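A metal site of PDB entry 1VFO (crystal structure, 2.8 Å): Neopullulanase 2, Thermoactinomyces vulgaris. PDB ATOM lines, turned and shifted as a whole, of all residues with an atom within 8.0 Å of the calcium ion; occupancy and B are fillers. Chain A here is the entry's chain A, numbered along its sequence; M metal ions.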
ATOM      1  N   PRO A 138       2.531 -31.524  17.028  1.00  0.00           N
ATOM      2  CA  PRO A 138       2.512 -30.483  18.064  1.00  0.00           C
ATOM      3  C   PRO A 138       1.449 -30.504  19.160  1.00  0.00           C
ATOM      4  O   PRO A 138       1.782 -30.524  20.353  1.00  0.00           O
ATOM      5  CB  PRO A 138       2.521 -29.188  17.260  1.00  0.00           C
ATOM      6  CG  PRO A 138       1.955 -29.595  15.944  1.00  0.00           C
ATOM      7  CD  PRO A 138       2.614 -30.901  15.705  1.00  0.00           C
ATOM      8  N   GLU A 139       0.177 -30.476  18.773  1.00  0.00           N
ATOM      9  CA  GLU A 139      -0.926 -30.455  19.738  1.00  0.00           C
ATOM     10  C   GLU A 139      -0.926 -31.646  20.717  1.00  0.00           C
ATOM     11  O   GLU A 139      -1.526 -31.570  21.786  1.00  0.00           O
ATOM     12  CB  GLU A 139      -2.263 -30.438  18.966  1.00  0.00           C
ATOM     13  CG  GLU A 139      -3.278 -29.347  19.380  1.00  0.00           C
ATOM     14  CD  GLU A 139      -3.815 -29.501  20.802  1.00  0.00           C
ATOM     15  OE1 GLU A 139      -3.595 -28.591  21.621  1.00  0.00           O
ATOM     16  OE2 GLU A 139      -4.459 -30.525  21.091  1.00  0.00           O
ATOM     17  N   ALA A 142       3.770 -32.352  23.698  1.00  0.00           N
ATOM     18  CA  ALA A 142       4.125 -31.829  25.031  1.00  0.00           C
ATOM     19  C   ALA A 142       3.554 -30.454  25.332  1.00  0.00           C
ATOM     20  O   ALA A 142       3.739 -29.499  24.579  1.00  0.00           O
ATOM     21  CB  ALA A 142       5.634 -31.791  25.164  1.00  0.00           C
ATOM     22  N   ASN A 143       2.840 -30.350  26.459  1.00  0.00           N
ATOM     23  CA  ASN A 143       2.273 -29.065  26.851  1.00  0.00           C
ATOM     24  C   ASN A 143       3.249 -28.363  27.802  1.00  0.00           C
ATOM     25  O   ASN A 143       3.123 -28.466  29.018  1.00  0.00           O
ATOM     26  CB  ASN A 143       0.941 -29.268  27.553  1.00  0.00           C
ATOM     27  CG  ASN A 143       0.141 -27.988  27.665  1.00  0.00           C
ATOM     28  OD1 ASN A 143       0.632 -26.903  27.322  1.00  0.00           O
ATOM     29  ND2 ASN A 143      -1.090 -28.096  28.147  1.00  0.00           N
ATOM     30  N   GLY A 144       4.217 -27.653  27.235  1.00  0.00           N
ATOM     31  CA  GLY A 144       5.207 -26.964  28.053  1.00  0.00           C
ATOM     32  C   GLY A 144       4.734 -25.631  28.596  1.00  0.00           C
ATOM     33  O   GLY A 144       5.321 -25.079  29.522  1.00  0.00           O
ATOM     34  N   ASP A 145       3.660 -25.122  28.016  1.00  0.00           N
ATOM     35  CA  ASP A 145       3.107 -23.854  28.419  1.00  0.00           C
ATOM     36  C   ASP A 145       1.588 -23.974  28.591  1.00  0.00           C
ATOM     37  O   ASP A 145       0.829 -23.943  27.615  1.00  0.00           O
ATOM     38  CB  ASP A 145       3.423 -22.806  27.361  1.00  0.00           C
ATOM     39  CG  ASP A 145       2.980 -21.417  27.765  1.00  0.00           C
ATOM     40  OD1 ASP A 145       2.375 -21.282  28.849  1.00  0.00           O
ATOM     41  OD2 ASP A 145       3.245 -20.467  26.998  1.00  0.00           O
ATOM     42  N   PRO A 146       1.139 -24.158  29.847  1.00  0.00           N
ATOM     43  CA  PRO A 146      -0.268 -24.295  30.232  1.00  0.00           C
ATOM     44  C   PRO A 146      -1.085 -23.030  29.944  1.00  0.00           C
ATOM     45  O   PRO A 146      -2.301 -23.104  29.763  1.00  0.00           O
ATOM     46  CB  PRO A 146      -0.194 -24.560  31.729  1.00  0.00           C
ATOM     47  CG  PRO A 146       1.089 -25.263  31.880  1.00  0.00           C
ATOM     48  CD  PRO A 146       2.020 -24.507  30.969  1.00  0.00           C
ATOM     49  N   SER A 147      -0.414 -21.876  29.911  1.00  0.00           N
ATOM     50  CA  SER A 147      -1.102 -20.610  29.684  1.00  0.00           C
ATOM     51  C   SER A 147      -1.654 -20.385  28.282  1.00  0.00           C
ATOM     52  O   SER A 147      -2.511 -19.524  28.093  1.00  0.00           O
ATOM     53  CB  SER A 147      -0.202 -19.439  30.066  1.00  0.00           C
ATOM     54  OG  SER A 147       0.798 -19.232  29.091  1.00  0.00           O
ATOM     55  N   ASN A 148      -1.170 -21.123  27.296  1.00  0.00           N
ATOM     56  CA  ASN A 148      -1.656 -20.929  25.935  1.00  0.00           C
ATOM     57  C   ASN A 148      -2.621 -22.018  25.477  1.00  0.00           C
ATOM     58  O   ASN A 148      -2.915 -22.114  24.294  1.00  0.00           O
ATOM     59  CB  ASN A 148      -0.498 -20.828  24.946  1.00  0.00           C
ATOM     60  CG  ASN A 148       0.352 -22.083  24.917  1.00  0.00           C
ATOM     61  OD1 ASN A 148      -0.124 -23.179  25.214  1.00  0.00           O
ATOM     62  ND2 ASN A 148       1.611 -21.923  24.534  1.00  0.00           N
ATOM     63  N   ASP A 149      -3.105 -22.826  26.415  1.00  0.00           N
ATOM     64  CA  ASP A 149      -4.026 -23.907  26.078  1.00  0.00           C
ATOM     65  C   ASP A 149      -5.343 -23.442  25.459  1.00  0.00           C
ATOM     66  O   ASP A 149      -5.877 -22.394  25.812  1.00  0.00           O
ATOM     67  CB  ASP A 149      -4.344 -24.739  27.310  1.00  0.00           C
ATOM     68  CG  ASP A 149      -3.149 -25.474  27.826  1.00  0.00           C
ATOM     69  OD1 ASP A 149      -3.329 -26.378  28.679  1.00  0.00           O
ATOM     70  OD2 ASP A 149      -2.027 -25.156  27.395  1.00  0.00           O
ATOM     71  N   PRO A 150      -5.896 -24.224  24.523  1.00  0.00           N
ATOM     72  CA  PRO A 150      -7.166 -23.841  23.910  1.00  0.00           C
ATOM     73  C   PRO A 150      -8.233 -24.002  24.973  1.00  0.00           C
ATOM     74  O   PRO A 150      -7.993 -24.624  26.013  1.00  0.00           O
ATOM     75  CB  PRO A 150      -7.340 -24.872  22.790  1.00  0.00           C
ATOM     76  CG  PRO A 150      -5.958 -25.389  22.535  1.00  0.00           C
ATOM     77  CD  PRO A 150      -5.369 -25.461  23.918  1.00  0.00           C
ATOM     78  N   THR A 153      -9.609 -27.863  27.056  1.00  0.00           N
ATOM     79  CA  THR A 153      -8.540 -28.843  26.961  1.00  0.00           C
ATOM     80  C   THR A 153      -8.912 -30.018  27.871  1.00  0.00           C
ATOM     81  O   THR A 153      -9.400 -29.805  28.974  1.00  0.00           O
ATOM     82  CB  THR A 153      -7.202 -28.239  27.443  1.00  0.00           C
ATOM     83  OG1 THR A 153      -6.731 -27.291  26.470  1.00  0.00           O
ATOM     84  CG2 THR A 153      -6.165 -29.312  27.650  1.00  0.00           C
ATOM     85  N   TRP A 156      -4.474 -34.801  30.341  1.00  0.00           N
ATOM     86  CA  TRP A 156      -3.331 -35.383  29.678  1.00  0.00           C
ATOM     87  C   TRP A 156      -3.004 -36.666  30.428  1.00  0.00           C
ATOM     88  O   TRP A 156      -2.077 -36.707  31.238  1.00  0.00           O
ATOM     89  CB  TRP A 156      -2.141 -34.428  29.719  1.00  0.00           C
ATOM     90  CG  TRP A 156      -1.079 -34.750  28.710  1.00  0.00           C
ATOM     91  CD1 TRP A 156      -0.285 -35.849  28.682  1.00  0.00           C
ATOM     92  CD2 TRP A 156      -0.710 -33.957  27.579  1.00  0.00           C
ATOM     93  NE1 TRP A 156       0.559 -35.801  27.605  1.00  0.00           N
ATOM     94  CE2 TRP A 156       0.317 -34.644  26.907  1.00  0.00           C
ATOM     95  CE3 TRP A 156      -1.156 -32.729  27.060  1.00  0.00           C
ATOM     96  CZ2 TRP A 156       0.923 -34.158  25.738  1.00  0.00           C
ATOM     97  CZ3 TRP A 156      -0.554 -32.238  25.904  1.00  0.00           C
ATOM     98  CH2 TRP A 156       0.471 -32.948  25.256  1.00  0.00           C
ATOM     99  N   TYR A 168      -5.505 -30.805  23.696  1.00  0.00           N
ATOM    100  CA  TYR A 168      -4.805 -31.258  24.900  1.00  0.00           C
ATOM    101  C   TYR A 168      -3.749 -30.292  25.425  1.00  0.00           C
ATOM    102  O   TYR A 168      -3.279 -30.451  26.555  1.00  0.00           O
ATOM    103  CB  TYR A 168      -4.181 -32.630  24.661  1.00  0.00           C
ATOM    104  CG  TYR A 168      -5.204 -33.739  24.612  1.00  0.00           C
ATOM    105  CD1 TYR A 168      -5.538 -34.456  25.748  1.00  0.00           C
ATOM    106  CD2 TYR A 168      -5.858 -34.045  23.412  1.00  0.00           C
ATOM    107  CE1 TYR A 168      -6.500 -35.459  25.707  1.00  0.00           C
ATOM    108  CE2 TYR A 168      -6.825 -35.051  23.355  1.00  0.00           C
ATOM    109  CZ  TYR A 168      -7.141 -35.754  24.506  1.00  0.00           C
ATOM    110  OH  TYR A 168      -8.107 -36.733  24.462  1.00  0.00           O
ATOM    111  N   GLY A 169      -3.363 -29.318  24.606  1.00  0.00           N
ATOM    112  CA  GLY A 169      -2.389 -28.331  25.043  1.00  0.00           C
ATOM    113  C   GLY A 169      -0.980 -28.383  24.495  1.00  0.00           C
ATOM    114  O   GLY A 169      -0.151 -27.549  24.862  1.00  0.00           O
ATOM    115  N   GLY A 170      -0.691 -29.341  23.625  1.00  0.00           N
ATOM    116  CA  GLY A 170       0.641 -29.437  23.056  1.00  0.00           C
ATOM    117  C   GLY A 170       1.128 -28.144  22.425  1.00  0.00           C
ATOM    118  O   GLY A 170       0.404 -27.501  21.676  1.00  0.00           O
ATOM    119  N   ASP A 171       2.363 -27.758  22.718  1.00  0.00           N
ATOM    120  CA  ASP A 171       2.937 -26.538  22.166  1.00  0.00           C
ATOM    121  C   ASP A 171       4.446 -26.669  21.891  1.00  0.00           C
ATOM    122  O   ASP A 171       5.080 -27.681  22.192  1.00  0.00           O
ATOM    123  CB  ASP A 171       2.688 -25.389  23.146  1.00  0.00           C
ATOM    124  CG  ASP A 171       3.075 -25.757  24.594  1.00  0.00           C
ATOM    125  OD1 ASP A 171       4.231 -26.183  24.820  1.00  0.00           O
ATOM    126  OD2 ASP A 171       2.212 -25.629  25.494  1.00  0.00           O
ATOM    127  N   LEU A 172       5.017 -25.616  21.316  1.00  0.00           N
ATOM    128  CA  LEU A 172       6.434 -25.587  20.992  1.00  0.00           C
ATOM    129  C   LEU A 172       7.309 -25.592  22.253  1.00  0.00           C
ATOM    130  O   LEU A 172       8.359 -26.240  22.297  1.00  0.00           O
ATOM    131  CB  LEU A 172       6.731 -24.359  20.109  1.00  0.00           C
ATOM    132  CG  LEU A 172       6.064 -24.426  18.718  1.00  0.00           C
ATOM    133  CD1 LEU A 172       6.258 -23.123  18.005  1.00  0.00           C
ATOM    134  CD2 LEU A 172       6.665 -25.563  17.907  1.00  0.00           C
ATOM    135  N   LYS A 173       6.874 -24.883  23.296  1.00  0.00           N
ATOM    136  CA  LYS A 173       7.635 -24.843  24.537  1.00  0.00           C
ATOM    137  C   LYS A 173       7.819 -26.290  25.032  1.00  0.00           C
ATOM    138  O   LYS A 173       8.897 -26.684  25.514  1.00  0.00           O
ATOM    139  CB  LYS A 173       6.906 -23.983  25.576  1.00  0.00           C
ATOM    140  CG  LYS A 173       7.585 -23.903  26.942  1.00  0.00           C
ATOM    141  CD  LYS A 173       9.047 -23.463  26.801  1.00  0.00           C
ATOM    142  CE  LYS A 173       9.807 -23.607  28.122  1.00  0.00           C
ATOM    143  NZ  LYS A 173       9.256 -22.698  29.146  1.00  0.00           N
ATOM    144  N   GLY A 174       6.762 -27.077  24.894  1.00  0.00           N
ATOM    145  CA  GLY A 174       6.837 -28.469  25.305  1.00  0.00           C
ATOM    146  C   GLY A 174       7.920 -29.192  24.522  1.00  0.00           C
ATOM    147  O   GLY A 174       8.675 -29.987  25.080  1.00  0.00           O
ATOM    148  N   PRO A 214      -1.127 -19.297  17.937  1.00  0.00           N
ATOM    149  CA  PRO A 214      -1.122 -18.841  19.327  1.00  0.00           C
ATOM    150  C   PRO A 214      -1.050 -19.925  20.403  1.00  0.00           C
ATOM    151  O   PRO A 214      -0.369 -19.756  21.429  1.00  0.00           O
ATOM    152  CB  PRO A 214      -2.400 -18.008  19.410  1.00  0.00           C
ATOM    153  CG  PRO A 214      -2.476 -17.396  18.069  1.00  0.00           C
ATOM    154  CD  PRO A 214      -2.167 -18.585  17.169  1.00  0.00           C
ATOM    155  N   GLN A 215      -1.743 -21.038  20.193  1.00  0.00           N
ATOM    156  CA  GLN A 215      -1.709 -22.108  21.174  1.00  0.00           C
ATOM    157  C   GLN A 215      -0.404 -22.901  21.099  1.00  0.00           C
ATOM    158  O   GLN A 215      -0.149 -23.736  21.958  1.00  0.00           O
ATOM    159  CB  GLN A 215      -2.918 -23.038  20.992  1.00  0.00           C
ATOM    160  CG  GLN A 215      -2.894 -23.862  19.738  1.00  0.00           C
ATOM    161  CD  GLN A 215      -4.237 -24.505  19.452  1.00  0.00           C
ATOM    162  OE1 GLN A 215      -5.253 -23.803  19.317  1.00  0.00           O
ATOM    163  NE2 GLN A 215      -4.259 -25.832  19.343  1.00  0.00           N
ATOM    164  N   PHE A 216       0.418 -22.627  20.084  1.00  0.00           N
ATOM    165  CA  PHE A 216       1.719 -23.285  19.916  1.00  0.00           C
ATOM    166  C   PHE A 216       2.883 -22.365  20.301  1.00  0.00           C
ATOM    167  O   PHE A 216       3.986 -22.832  20.590  1.00  0.00           O
ATOM    168  CB  PHE A 216       1.929 -23.757  18.462  1.00  0.00           C
ATOM    169  CG  PHE A 216       1.120 -24.972  18.076  1.00  0.00           C
ATOM    170  CD1 PHE A 216       0.742 -25.923  19.030  1.00  0.00           C
ATOM    171  CD2 PHE A 216       0.760 -25.194  16.741  1.00  0.00           C
ATOM    172  CE1 PHE A 216       0.031 -27.065  18.653  1.00  0.00           C
ATOM    173  CE2 PHE A 216       0.062 -26.334  16.359  1.00  0.00           C
ATOM    174  CZ  PHE A 216      -0.316 -27.267  17.322  1.00  0.00           C
ATOM    175  N   GLY A 217       2.643 -21.054  20.292  1.00  0.00           N
ATOM    176  CA  GLY A 217       3.685 -20.124  20.661  1.00  0.00           C
ATOM    177  C   GLY A 217       3.750 -18.871  19.803  1.00  0.00           C
ATOM    178  O   GLY A 217       2.730 -18.374  19.338  1.00  0.00           O
HETATM  179 CA    CA M   1      -0.215 -25.348  25.895  1.00  0.00          CA
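OD1 of Asn 148 lies close to O of Gln 215, at 3.3 Å.
The backbone NH (N) of Gly 169 sits at hydrogen-bond distance from the side-chain carboxylate (OE1) of Glu 139 (3.1 Å).
OD1 of Asp 145 sits at hydrogen-bond distance from OG of Ser 147.
N of Gly 144 sits at hydrogen-bond distance from OD1 of Asp 171 (2.8 Å).
The backbone NH of Asp 171 lies within hydrogen-bond range of the backbone carbonyl oxygen of Ala 142 (2.9 Å).
The backbone NH (N) of Gly 174 sits at hydrogen-bond distance from the side-chain carboxylate (OD1) of Asp 171, at 2.7 Å.
OD1 of Asp 171 sits at hydrogen-bond distance from N of Lys 173 (3.3 Å).
Of the 24 residues printed, 6 come within 4 Å of the calcium ion.
The calcium ion is bound by OD1 of Asn 143 (2.3 Å), OD1 of Asn 148 (2.3 Å), OD2 of Asp 149 (2.4 Å), O of Gly 169 (2.4 Å), O of Asp 145 (2.5 Å) and OD2 of Asp 171 (2.5 Å).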
